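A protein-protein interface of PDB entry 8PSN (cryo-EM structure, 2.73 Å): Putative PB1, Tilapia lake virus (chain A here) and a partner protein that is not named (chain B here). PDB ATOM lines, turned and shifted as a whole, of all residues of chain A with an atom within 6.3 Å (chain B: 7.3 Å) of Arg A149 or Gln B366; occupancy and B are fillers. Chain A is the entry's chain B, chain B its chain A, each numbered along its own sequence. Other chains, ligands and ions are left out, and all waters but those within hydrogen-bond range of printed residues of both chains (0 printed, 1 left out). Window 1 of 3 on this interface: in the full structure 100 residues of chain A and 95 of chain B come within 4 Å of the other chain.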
ATOM      1  N   TRP A   2      18.609  29.822  20.212  1.00  0.00           N
ATOM      2  CA  TRP A   2      17.487  29.091  20.789  1.00  0.00           C
ATOM      3  C   TRP A   2      17.826  27.626  21.023  1.00  0.00           C
ATOM      4  O   TRP A   2      17.186  26.976  21.856  1.00  0.00           O
ATOM      5  CB  TRP A   2      16.257  29.193  19.880  1.00  0.00           C
ATOM      6  CG  TRP A   2      16.564  29.000  18.424  1.00  0.00           C
ATOM      7  CD1 TRP A   2      16.727  29.977  17.487  1.00  0.00           C
ATOM      8  CD2 TRP A   2      16.753  27.755  17.741  1.00  0.00           C
ATOM      9  NE1 TRP A   2      17.004  29.419  16.263  1.00  0.00           N
ATOM     10  CE2 TRP A   2      17.025  28.056  16.392  1.00  0.00           C
ATOM     11  CE3 TRP A   2      16.716  26.415  18.137  1.00  0.00           C
ATOM     12  CZ2 TRP A   2      17.258  27.068  15.441  1.00  0.00           C
ATOM     13  CZ3 TRP A   2      16.948  25.437  17.191  1.00  0.00           C
ATOM     14  CH2 TRP A   2      17.216  25.768  15.858  1.00  0.00           C
ATOM     15  N   CYS A   9      12.290  26.443  24.829  1.00  0.00           N
ATOM     16  CA  CYS A   9      12.265  27.679  24.055  1.00  0.00           C
ATOM     17  C   CYS A   9      11.754  27.379  22.655  1.00  0.00           C
ATOM     18  O   CYS A   9      12.298  26.507  21.971  1.00  0.00           O
ATOM     19  CB  CYS A   9      13.658  28.313  23.988  1.00  0.00           C
ATOM     20  SG  CYS A   9      13.689  29.949  23.231  1.00  0.00           S
ATOM     21  N   LYS A  10      10.721  28.102  22.233  1.00  0.00           N
ATOM     22  CA  LYS A  10      10.163  27.955  20.895  1.00  0.00           C
ATOM     23  C   LYS A  10      10.792  28.897  19.877  1.00  0.00           C
ATOM     24  O   LYS A  10      10.444  28.823  18.694  1.00  0.00           O
ATOM     25  CB  LYS A  10       8.652  28.191  20.921  1.00  0.00           C
ATOM     26  CG  LYS A  10       7.854  27.088  21.593  1.00  0.00           C
ATOM     27  CD  LYS A  10       6.673  26.632  20.738  1.00  0.00           C
ATOM     28  CE  LYS A  10       5.759  27.784  20.331  1.00  0.00           C
ATOM     29  NZ  LYS A  10       4.650  27.324  19.453  1.00  0.00           N
ATOM     30  N   GLY A  11      11.700  29.773  20.295  1.00  0.00           N
ATOM     31  CA  GLY A  11      12.301  30.721  19.379  1.00  0.00           C
ATOM     32  C   GLY A  11      11.309  31.716  18.811  1.00  0.00           C
ATOM     33  O   GLY A  11      11.291  31.963  17.603  1.00  0.00           O
ATOM     34  N   ASN A  12      10.479  32.296  19.676  1.00  0.00           N
ATOM     35  CA  ASN A  12       9.476  33.272  19.271  1.00  0.00           C
ATOM     36  C   ASN A  12       9.972  34.710  19.379  1.00  0.00           C
ATOM     37  O   ASN A  12       9.163  35.638  19.281  1.00  0.00           O
ATOM     38  CB  ASN A  12       8.212  33.110  20.120  1.00  0.00           C
ATOM     39  CG  ASN A  12       7.357  31.943  19.678  1.00  0.00           C
ATOM     40  OD1 ASN A  12       7.712  31.210  18.757  1.00  0.00           O
ATOM     41  ND2 ASN A  12       6.219  31.765  20.336  1.00  0.00           N
ATOM     42  N   LEU A  13      11.275  34.918  19.574  1.00  0.00           N
ATOM     43  CA  LEU A  13      11.774  36.266  19.824  1.00  0.00           C
ATOM     44  C   LEU A  13      11.648  37.159  18.595  1.00  0.00           C
ATOM     45  O   LEU A  13      11.454  38.372  18.735  1.00  0.00           O
ATOM     46  CB  LEU A  13      13.228  36.206  20.292  1.00  0.00           C
ATOM     47  CG  LEU A  13      13.497  35.547  21.653  1.00  0.00           C
ATOM     48  CD1 LEU A  13      14.795  36.067  22.245  1.00  0.00           C
ATOM     49  CD2 LEU A  13      12.351  35.755  22.635  1.00  0.00           C
ATOM     50  N   LEU A  14      11.755  36.598  17.397  1.00  0.00           N
ATOM     51  CA  LEU A  14      11.602  37.358  16.166  1.00  0.00           C
ATOM     52  C   LEU A  14      10.181  37.225  15.632  1.00  0.00           C
ATOM     53  O   LEU A  14       9.426  36.329  16.016  1.00  0.00           O
ATOM     54  CB  LEU A  14      12.601  36.891  15.104  1.00  0.00           C
ATOM     55  CG  LEU A  14      14.070  36.841  15.527  1.00  0.00           C
ATOM     56  CD1 LEU A  14      14.926  36.321  14.385  1.00  0.00           C
ATOM     57  CD2 LEU A  14      14.551  38.209  15.978  1.00  0.00           C
ATOM     58  N   SER A  15       9.822  38.137  14.732  1.00  0.00           N
ATOM     59  CA  SER A  15       8.501  38.122  14.126  1.00  0.00           C
ATOM     60  C   SER A  15       8.342  36.884  13.245  1.00  0.00           C
ATOM     61  O   SER A  15       9.273  36.100  13.045  1.00  0.00           O
ATOM     62  CB  SER A  15       8.274  39.396  13.315  1.00  0.00           C
ATOM     63  OG  SER A  15       8.516  40.549  14.098  1.00  0.00           O
ATOM     64  N   GLY A  16       7.137  36.710  12.710  1.00  0.00           N
ATOM     65  CA  GLY A  16       6.836  35.588  11.855  1.00  0.00           C
ATOM     66  C   GLY A  16       7.175  35.854  10.403  1.00  0.00           C
ATOM     67  O   GLY A  16       7.607  36.949  10.031  1.00  0.00           O
ATOM     68  N   PRO A  17       6.987  34.848   9.553  1.00  0.00           N
ATOM     69  CA  PRO A  17       7.274  35.025   8.125  1.00  0.00           C
ATOM     70  C   PRO A  17       6.290  35.971   7.458  1.00  0.00           C
ATOM     71  O   PRO A  17       5.134  36.098   7.869  1.00  0.00           O
ATOM     72  CB  PRO A  17       7.147  33.607   7.552  1.00  0.00           C
ATOM     73  CG  PRO A  17       6.957  32.692   8.721  1.00  0.00           C
ATOM     74  CD  PRO A  17       6.459  33.510   9.853  1.00  0.00           C
ATOM     75  N   GLN A 147       2.840  36.002   9.037  1.00  0.00           N
ATOM     76  CA  GLN A 147       3.253  36.258  10.416  1.00  0.00           C
ATOM     77  C   GLN A 147       2.902  35.094  11.339  1.00  0.00           C
ATOM     78  O   GLN A 147       2.695  35.283  12.539  1.00  0.00           O
ATOM     79  CB  GLN A 147       2.636  37.555  10.945  1.00  0.00           C
ATOM     80  CG  GLN A 147       3.067  38.799  10.184  1.00  0.00           C
ATOM     81  CD  GLN A 147       4.319  39.431  10.757  1.00  0.00           C
ATOM     82  OE1 GLN A 147       5.301  39.644  10.046  1.00  0.00           O
ATOM     83  NE2 GLN A 147       4.290  39.742  12.047  1.00  0.00           N
ATOM     84  N   GLU A 148       2.833  33.884  10.791  1.00  0.00           N
ATOM     85  CA  GLU A 148       2.602  32.677  11.575  1.00  0.00           C
ATOM     86  C   GLU A 148       3.954  32.033  11.856  1.00  0.00           C
ATOM     87  O   GLU A 148       4.575  31.458  10.956  1.00  0.00           O
ATOM     88  CB  GLU A 148       1.677  31.712  10.838  1.00  0.00           C
ATOM     89  CG  GLU A 148       0.287  31.613  11.436  1.00  0.00           C
ATOM     90  CD  GLU A 148      -0.503  30.443  10.882  1.00  0.00           C
ATOM     91  OE1 GLU A 148      -0.819  30.457   9.675  1.00  0.00           O
ATOM     92  OE2 GLU A 148      -0.807  29.511  11.654  1.00  0.00           O
ATOM     93  N   ARG A 149       4.409  32.134  13.102  1.00  0.00           N
ATOM     94  CA  ARG A 149       5.722  31.619  13.460  1.00  0.00           C
ATOM     95  C   ARG A 149       5.796  30.119  13.208  1.00  0.00           C
ATOM     96  O   ARG A 149       4.878  29.371  13.555  1.00  0.00           O
ATOM     97  CB  ARG A 149       6.024  31.927  14.925  1.00  0.00           C
ATOM     98  CG  ARG A 149       6.648  33.292  15.148  1.00  0.00           C
ATOM     99  CD  ARG A 149       6.427  33.781  16.564  1.00  0.00           C
ATOM    100  NE  ARG A 149       6.954  35.127  16.759  1.00  0.00           N
ATOM    101  CZ  ARG A 149       6.351  36.085  17.453  1.00  0.00           C
ATOM    102  NH1 ARG A 149       5.190  35.884  18.052  1.00  0.00           N
ATOM    103  NH2 ARG A 149       6.932  37.277  17.548  1.00  0.00           N
ATOM    104  N   GLY A 150       6.899  29.682  12.605  1.00  0.00           N
ATOM    105  CA  GLY A 150       7.099  28.279  12.316  1.00  0.00           C
ATOM    106  C   GLY A 150       6.439  27.786  11.050  1.00  0.00           C
ATOM    107  O   GLY A 150       6.387  26.570  10.834  1.00  0.00           O
ATOM    108  N   LYS A 151       5.933  28.681  10.206  1.00  0.00           N
ATOM    109  CA  LYS A 151       5.281  28.314   8.950  1.00  0.00           C
ATOM    110  C   LYS A 151       5.937  29.105   7.827  1.00  0.00           C
ATOM    111  O   LYS A 151       5.409  30.133   7.382  1.00  0.00           O
ATOM    112  CB  LYS A 151       3.775  28.573   9.009  1.00  0.00           C
ATOM    113  CG  LYS A 151       3.004  27.497   9.762  1.00  0.00           C
ATOM    114  CD  LYS A 151       3.083  26.142   9.080  1.00  0.00           C
ATOM    115  CE  LYS A 151       2.242  25.109   9.817  1.00  0.00           C
ATOM    116  NZ  LYS A 151       2.320  23.765   9.183  1.00  0.00           N
ATOM    117  N   PRO A 152       7.095  28.650   7.339  1.00  0.00           N
ATOM    118  CA  PRO A 152       7.778  29.404   6.274  1.00  0.00           C
ATOM    119  C   PRO A 152       6.905  29.641   5.056  1.00  0.00           C
ATOM    120  O   PRO A 152       6.983  30.712   4.442  1.00  0.00           O
ATOM    121  CB  PRO A 152       8.991  28.522   5.945  1.00  0.00           C
ATOM    122  CG  PRO A 152       9.174  27.638   7.118  1.00  0.00           C
ATOM    123  CD  PRO A 152       7.830  27.435   7.727  1.00  0.00           C
ATOM    124  N   CYS A 346       7.322  30.312  25.457  1.00  0.00           N
ATOM    125  CA  CYS A 346       6.694  30.924  24.295  1.00  0.00           C
ATOM    126  C   CYS A 346       6.829  32.440  24.285  1.00  0.00           C
ATOM    127  O   CYS A 346       6.160  33.104  23.488  1.00  0.00           O
ATOM    128  CB  CYS A 346       5.217  30.532  24.233  1.00  0.00           C
ATOM    129  SG  CYS A 346       4.293  30.873  25.747  1.00  0.00           S
ATOM    130  N   ALA A 348       7.534  36.022  23.384  1.00  0.00           N
ATOM    131  CA  ALA A 348       7.722  36.599  22.062  1.00  0.00           C
ATOM    132  C   ALA A 348       8.279  38.010  22.179  1.00  0.00           C
ATOM    133  O   ALA A 348       7.892  38.769  23.073  1.00  0.00           O
ATOM    134  CB  ALA A 348       6.405  36.623  21.283  1.00  0.00           C
ATOM    135  N   GLY A 349       9.188  38.355  21.275  1.00  0.00           N
ATOM    136  CA  GLY A 349       9.749  39.688  21.251  1.00  0.00           C
ATOM    137  C   GLY A 349       8.768  40.709  20.710  1.00  0.00           C
ATOM    138  O   GLY A 349       7.710  40.388  20.169  1.00  0.00           O
ATOM    139  N   VAL A 350       9.134  41.972  20.867  1.00  0.00           N
ATOM    140  CA  VAL A 350       8.320  43.104  20.435  1.00  0.00           C
ATOM    141  C   VAL A 350       9.068  43.818  19.312  1.00  0.00           C
ATOM    142  O   VAL A 350      10.191  44.289  19.532  1.00  0.00           O
ATOM    143  CB  VAL A 350       8.024  44.065  21.597  1.00  0.00           C
ATOM    144  CG1 VAL A 350       7.045  45.143  21.160  1.00  0.00           C
ATOM    145  CG2 VAL A 350       7.482  43.300  22.791  1.00  0.00           C
ATOM    146  N   PRO A 351       8.506  43.919  18.111  1.00  0.00           N
ATOM    147  CA  PRO A 351       9.173  44.661  17.039  1.00  0.00           C
ATOM    148  C   PRO A 351       8.943  46.161  17.174  1.00  0.00           C
ATOM    149  O   PRO A 351       8.127  46.630  17.968  1.00  0.00           O
ATOM    150  CB  PRO A 351       8.522  44.110  15.769  1.00  0.00           C
ATOM    151  CG  PRO A 351       7.167  43.678  16.197  1.00  0.00           C
ATOM    152  CD  PRO A 351       7.232  43.329  17.661  1.00  0.00           C
ATOM    153  N   GLN B 311      13.078  44.226  13.391  1.00  0.00           N
ATOM    154  CA  GLN B 311      13.621  43.336  14.406  1.00  0.00           C
ATOM    155  C   GLN B 311      14.587  44.085  15.314  1.00  0.00           C
ATOM    156  O   GLN B 311      15.325  44.968  14.871  1.00  0.00           O
ATOM    157  CB  GLN B 311      14.330  42.151  13.749  1.00  0.00           C
ATOM    158  CG  GLN B 311      13.436  41.305  12.853  1.00  0.00           C
ATOM    159  CD  GLN B 311      12.094  40.998  13.483  1.00  0.00           C
ATOM    160  OE1 GLN B 311      12.023  40.492  14.602  1.00  0.00           O
ATOM    161  NE2 GLN B 311      11.020  41.306  12.768  1.00  0.00           N
ATOM    162  N   ARG B 359      11.980  33.440   7.998  1.00  0.00           N
ATOM    163  CA  ARG B 359      12.040  32.987   9.387  1.00  0.00           C
ATOM    164  C   ARG B 359      11.919  31.468   9.478  1.00  0.00           C
ATOM    165  O   ARG B 359      11.217  30.929  10.335  1.00  0.00           O
ATOM    166  CB  ARG B 359      10.960  33.665  10.230  1.00  0.00           C
ATOM    167  CG  ARG B 359      11.041  35.180  10.253  1.00  0.00           C
ATOM    168  CD  ARG B 359      12.177  35.669  11.133  1.00  0.00           C
ATOM    169  NE  ARG B 359      12.787  36.884  10.610  1.00  0.00           N
ATOM    170  CZ  ARG B 359      12.253  38.094  10.707  1.00  0.00           C
ATOM    171  NH1 ARG B 359      11.090  38.291  11.306  1.00  0.00           N
ATOM    172  NH2 ARG B 359      12.899  39.133  10.187  1.00  0.00           N
ATOM    173  N   VAL B 360      12.617  30.767   8.581  1.00  0.00           N
ATOM    174  CA  VAL B 360      12.586  29.310   8.591  1.00  0.00           C
ATOM    175  C   VAL B 360      13.188  28.751   9.869  1.00  0.00           C
ATOM    176  O   VAL B 360      12.856  27.632  10.271  1.00  0.00           O
ATOM    177  CB  VAL B 360      13.313  28.748   7.352  1.00  0.00           C
ATOM    178  CG1 VAL B 360      14.799  29.058   7.414  1.00  0.00           C
ATOM    179  CG2 VAL B 360      13.081  27.249   7.236  1.00  0.00           C
ATOM    180  N   SER B 361      14.073  29.506  10.524  1.00  0.00           N
ATOM    181  CA  SER B 361      14.677  29.032  11.763  1.00  0.00           C
ATOM    182  C   SER B 361      13.645  28.808  12.858  1.00  0.00           C
ATOM    183  O   SER B 361      13.904  28.039  13.787  1.00  0.00           O
ATOM    184  CB  SER B 361      15.730  30.030  12.247  1.00  0.00           C
ATOM    185  OG  SER B 361      15.118  31.186  12.788  1.00  0.00           O
ATOM    186  N   GLN B 362      12.487  29.468  12.778  1.00  0.00           N
ATOM    187  CA  GLN B 362      11.454  29.273  13.789  1.00  0.00           C
ATOM    188  C   GLN B 362      10.879  27.863  13.731  1.00  0.00           C
ATOM    189  O   GLN B 362      10.602  27.257  14.772  1.00  0.00           O
ATOM    190  CB  GLN B 362      10.348  30.312  13.611  1.00  0.00           C
ATOM    191  CG  GLN B 362      10.504  31.529  14.507  1.00  0.00           C
ATOM    192  CD  GLN B 362       9.972  32.799  13.875  1.00  0.00           C
ATOM    193  OE1 GLN B 362       9.286  32.761  12.855  1.00  0.00           O
ATOM    194  NE2 GLN B 362      10.279  33.935  14.487  1.00  0.00           N
ATOM    195  N   ALA B 363      10.683  27.326  12.524  1.00  0.00           N
ATOM    196  CA  ALA B 363      10.200  25.955  12.400  1.00  0.00           C
ATOM    197  C   ALA B 363      11.200  24.968  12.988  1.00  0.00           C
ATOM    198  O   ALA B 363      10.819  24.031  13.701  1.00  0.00           O
ATOM    199  CB  ALA B 363       9.924  25.629  10.934  1.00  0.00           C
ATOM    200  N   VAL B 364      12.488  25.168  12.703  1.00  0.00           N
ATOM    201  CA  VAL B 364      13.514  24.300  13.271  1.00  0.00           C
ATOM    202  C   VAL B 364      13.529  24.425  14.787  1.00  0.00           C
ATOM    203  O   VAL B 364      13.691  23.431  15.501  1.00  0.00           O
ATOM    204  CB  VAL B 364      14.891  24.623  12.662  1.00  0.00           C
ATOM    205  CG1 VAL B 364      15.941  23.653  13.180  1.00  0.00           C
ATOM    206  CG2 VAL B 364      14.827  24.574  11.144  1.00  0.00           C
ATOM    207  N   ALA B 365      13.369  25.644  15.303  1.00  0.00           N
ATOM    208  CA  ALA B 365      13.359  25.840  16.748  1.00  0.00           C
ATOM    209  C   ALA B 365      12.190  25.111  17.399  1.00  0.00           C
ATOM    210  O   ALA B 365      12.354  24.459  18.436  1.00  0.00           O
ATOM    211  CB  ALA B 365      13.305  27.332  17.072  1.00  0.00           C
ATOM    212  N   GLN B 366      11.000  25.210  16.804  1.00  0.00           N
ATOM    213  CA  GLN B 366       9.836  24.525  17.362  1.00  0.00           C
ATOM    214  C   GLN B 366      10.011  23.013  17.314  1.00  0.00           C
ATOM    215  O   GLN B 366       9.701  22.307  18.285  1.00  0.00           O
ATOM    216  CB  GLN B 366       8.576  24.944  16.607  1.00  0.00           C
ATOM    217  CG  GLN B 366       8.176  26.393  16.831  1.00  0.00           C
ATOM    218  CD  GLN B 366       7.101  26.856  15.871  1.00  0.00           C
ATOM    219  OE1 GLN B 366       6.577  26.070  15.083  1.00  0.00           O
ATOM    220  NE2 GLN B 366       6.768  28.139  15.930  1.00  0.00           N
ATOM    221  N   HIS B 367      10.513  22.492  16.192  1.00  0.00           N
ATOM    222  CA  HIS B 367      10.722  21.053  16.093  1.00  0.00           C
ATOM    223  C   HIS B 367      11.785  20.584  17.077  1.00  0.00           C
ATOM    224  O   HIS B 367      11.673  19.493  17.642  1.00  0.00           O
ATOM    225  CB  HIS B 367      11.102  20.669  14.665  1.00  0.00           C
ATOM    226  CG  HIS B 367      10.745  19.259  14.310  1.00  0.00           C
ATOM    227  ND1 HIS B 367       9.473  18.752  14.469  1.00  0.00           N
ATOM    228  CD2 HIS B 367      11.494  18.246  13.815  1.00  0.00           C
ATOM    229  CE1 HIS B 367       9.453  17.490  14.082  1.00  0.00           C
ATOM    230  NE2 HIS B 367      10.666  17.158  13.680  1.00  0.00           N
ATOM    231  N   PHE B 368      12.824  21.390  17.299  1.00  0.00           N
ATOM    232  CA  PHE B 368      13.855  21.016  18.260  1.00  0.00           C
ATOM    233  C   PHE B 368      13.321  21.057  19.685  1.00  0.00           C
ATOM    234  O   PHE B 368      13.717  20.243  20.525  1.00  0.00           O
ATOM    235  CB  PHE B 368      15.063  21.940  18.109  1.00  0.00           C
ATOM    236  CG  PHE B 368      16.271  21.493  18.881  1.00  0.00           C
ATOM    237  CD1 PHE B 368      16.741  20.197  18.770  1.00  0.00           C
ATOM    238  CD2 PHE B 368      16.937  22.372  19.714  1.00  0.00           C
ATOM    239  CE1 PHE B 368      17.849  19.787  19.477  1.00  0.00           C
ATOM    240  CE2 PHE B 368      18.047  21.967  20.422  1.00  0.00           C
ATOM    241  CZ  PHE B 368      18.503  20.673  20.304  1.00  0.00           C
ATOM    242  N   ASN B 369      12.427  22.002  19.980  1.00  0.00           N
ATOM    243  CA  ASN B 369      11.766  22.008  21.281  1.00  0.00           C
ATOM    244  C   ASN B 369      10.967  20.728  21.482  1.00  0.00           C
ATOM    245  O   ASN B 369      11.059  20.074  22.531  1.00  0.00           O
ATOM    246  CB  ASN B 369      10.862  23.237  21.395  1.00  0.00           C
ATOM    247  CG  ASN B 369      10.281  23.409  22.783  1.00  0.00           C
ATOM    248  OD1 ASN B 369      10.996  23.726  23.732  1.00  0.00           O
ATOM    249  ND2 ASN B 369       8.977  23.204  22.908  1.00  0.00           N
ATOM    250  N   ARG B 370      10.194  20.337  20.466  1.00  0.00           N
ATOM    251  CA  ARG B 370       9.458  19.079  20.545  1.00  0.00           C
ATOM    252  C   ARG B 370      10.408  17.902  20.730  1.00  0.00           C
ATOM    253  O   ARG B 370      10.133  16.986  21.514  1.00  0.00           O
ATOM    254  CB  ARG B 370       8.615  18.885  19.286  1.00  0.00           C
ATOM    255  CG  ARG B 370       7.270  19.578  19.317  1.00  0.00           C
ATOM    256  CD  ARG B 370       6.383  19.089  18.188  1.00  0.00           C
ATOM    257  NE  ARG B 370       6.872  19.508  16.881  1.00  0.00           N
ATOM    258  CZ  ARG B 370       6.553  20.650  16.287  1.00  0.00           C
ATOM    259  NH1 ARG B 370       5.745  21.528  16.860  1.00  0.00           N
ATOM    260  NH2 ARG B 370       7.057  20.920  15.087  1.00  0.00           N
ATOM    261  N   HIS B 371      11.529  17.913  20.012  1.00  0.00           N
ATOM    262  CA  HIS B 371      12.505  16.832  20.103  1.00  0.00           C
ATOM    263  C   HIS B 371      13.080  16.730  21.509  1.00  0.00           C
ATOM    264  O   HIS B 371      13.238  15.628  22.047  1.00  0.00           O
ATOM    265  CB  HIS B 371      13.610  17.073  19.073  1.00  0.00           C
ATOM    266  CG  HIS B 371      14.674  16.021  19.052  1.00  0.00           C
ATOM    267  ND1 HIS B 371      15.818  16.143  18.293  1.00  0.00           N
ATOM    268  CD2 HIS B 371      14.772  14.832  19.688  1.00  0.00           C
ATOM    269  CE1 HIS B 371      16.574  15.075  18.465  1.00  0.00           C
ATOM    270  NE2 HIS B 371      15.963  14.264  19.307  1.00  0.00           N
ATOM    271  N   ARG B 372      13.404  17.870  22.119  1.00  0.00           N
ATOM    272  CA  ARG B 372      13.965  17.856  23.465  1.00  0.00           C
ATOM    273  C   ARG B 372      12.934  17.400  24.488  1.00  0.00           C
ATOM    274  O   ARG B 372      13.278  16.716  25.459  1.00  0.00           O
ATOM    275  CB  ARG B 372      14.499  19.242  23.827  1.00  0.00           C
ATOM    276  CG  ARG B 372      15.826  19.585  23.175  1.00  0.00           C
ATOM    277  CD  ARG B 372      16.216  21.027  23.441  1.00  0.00           C
ATOM    278  NE  ARG B 372      16.515  21.258  24.849  1.00  0.00           N
ATOM    279  CZ  ARG B 372      16.424  22.433  25.456  1.00  0.00           C
ATOM    280  NH1 ARG B 372      16.053  23.523  24.804  1.00  0.00           N
ATOM    281  NH2 ARG B 372      16.715  22.517  26.750  1.00  0.00           N
ATOM    282  N   PHE B 382       8.629  12.035  12.579  1.00  0.00           N
ATOM    283  CA  PHE B 382       9.181  13.129  13.369  1.00  0.00           C
ATOM    284  C   PHE B 382      10.490  13.628  12.771  1.00  0.00           C
ATOM    285  O   PHE B 382      10.750  14.836  12.748  1.00  0.00           O
ATOM    286  CB  PHE B 382       9.387  12.679  14.814  1.00  0.00           C
ATOM    287  CG  PHE B 382       9.775  13.791  15.745  1.00  0.00           C
ATOM    288  CD1 PHE B 382       8.808  14.565  16.360  1.00  0.00           C
ATOM    289  CD2 PHE B 382      11.107  14.064  16.002  1.00  0.00           C
ATOM    290  CE1 PHE B 382       9.162  15.589  17.214  1.00  0.00           C
ATOM    291  CE2 PHE B 382      11.466  15.086  16.855  1.00  0.00           C
ATOM    292  CZ  PHE B 382      10.491  15.849  17.462  1.00  0.00           C
ATOM    293  N   TYR B 386      12.451  17.868  10.153  1.00  0.00           N
ATOM    294  CA  TYR B 386      13.672  18.642   9.981  1.00  0.00           C
ATOM    295  C   TYR B 386      14.007  18.901   8.518  1.00  0.00           C
ATOM    296  O   TYR B 386      15.005  19.571   8.237  1.00  0.00           O
ATOM    297  CB  TYR B 386      14.847  17.926  10.654  1.00  0.00           C
ATOM    298  CG  TYR B 386      14.904  18.103  12.154  1.00  0.00           C
ATOM    299  CD1 TYR B 386      15.055  19.361  12.720  1.00  0.00           C
ATOM    300  CD2 TYR B 386      14.809  17.009  13.004  1.00  0.00           C
ATOM    301  CE1 TYR B 386      15.107  19.526  14.089  1.00  0.00           C
ATOM    302  CE2 TYR B 386      14.861  17.165  14.375  1.00  0.00           C
ATOM    303  CZ  TYR B 386      15.011  18.425  14.912  1.00  0.00           C
ATOM    304  OH  TYR B 386      15.063  18.584  16.275  1.00  0.00           O
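Among the printed residues, pairs that only touch across the chains: Gly A11 with Gln B362 (3.2 Å), Leu A14 with Gln B311 (3.5 Å), Arg A149 with Gln B362 (3.5 Å), Trp A2 with Ala B365 (3.5 Å), Gly A150 with Gln B366 (3.6 Å), Lys A10 with Ala B365 (3.6 Å), Trp A2 with Val B364 (3.6 Å), Gly A150 with Gln B362 (3.6 Å), Gly A150 with Ala B363 (3.7 Å), Lys A10 with Gln B366 (3.8 Å), Trp A2 with Ser B361 (3.9 Å), Gly A16 with Arg B359 (3.9 Å), Gly A16 with Gln B362 (3.9 Å), Pro A152 with Val B360 (3.9 Å) and Trp A2 with Phe B368 (3.97 Å).
Of chain B, only Gln B362 (3.5 Å) and Gln B366 (3.3 Å) come within 4 Å of Arg A149.
Of chain A, only Lys A10 (3.8 Å), Arg A149 (3.3 Å) and Gly A150 (3.6 Å) come within 4 Å of Gln B366.
Printed residues of chain B within 4 Å of Gly A150: Gln B362, Ala B363 and Gln B366.
Of the printed residues of chain A, Ala B363 touches Gly A150.
Printed residues of chain A within 4 Å of Asn B369: Cys A9 (3.2 Å).
Of the printed residues of chain B, Leu A14 touches Gln B311 and Gln B362.
Printed residues of chain B within 4 Å of Gly A11: Gln B362 (3.2 Å).
Pro A17 touches none of the printed residues of chain B.
The nearest residue of chain B that does not touch Arg A149 is Ala B363 (5.7 Å).
The nearest printed residue of chain A that does not touch Phe B368 is Cys A9 (6.0 Å).
Hydrophobic or aromatic side chains of chain B that line the printed part of chain A: Val B360, Ala B363, Val B364, Ala B365 and Phe B368.
Of the 21 printed residues of chain A, 10 touch a printed residue of chain B.
Printed residues of chain A that touch a printed residue of chain B: Trp A2, Cys A9, Lys A10, Gly A11, Leu A14, Ser A15, Gly A16, Arg A149, Gly A150 and Pro A152.
Along chain A the printed residues that touch a printed residue of chain B span positions 2 to 152.
The guanidinium group (NH1) of Arg B359 sits close to the side-chain amide nitrogen (NE2) of Gln B311 (3.4 Å).
The backbone NH of Gly A11 lies close to the side-chain sulfur of Cys A9 (3.6 Å).
The backbone carbonyl oxygen (O) of Asn A12 lies within hydrogen-bond range of the guanidinium group (NH2) of Arg A149.
NE of Arg A149 lies within hydrogen-bond range of O of Leu A14 (2.8 Å).
O of Leu A14 is in hydrogen-bond range of NE2 of Gln B362, at 3.0 Å.
The side-chain amide oxygen (OD1) of Asn B369 lies within hydrogen-bond range of the backbone NH (N) of Cys A9, at 3.2 Å.
The side-chain amide nitrogen (NE2) of Gln B362 is in hydrogen-bond range of the backbone carbonyl oxygen (O) of Ser A15, 2.8 Å away.
NH1 of Arg B359 lies within hydrogen-bond range of O of Ser A15.
OG of Ser A15 lies within hydrogen-bond range of NE2 of Gln B311.
NE2 of Gln B366 lies within hydrogen-bond range of O of Arg A149.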
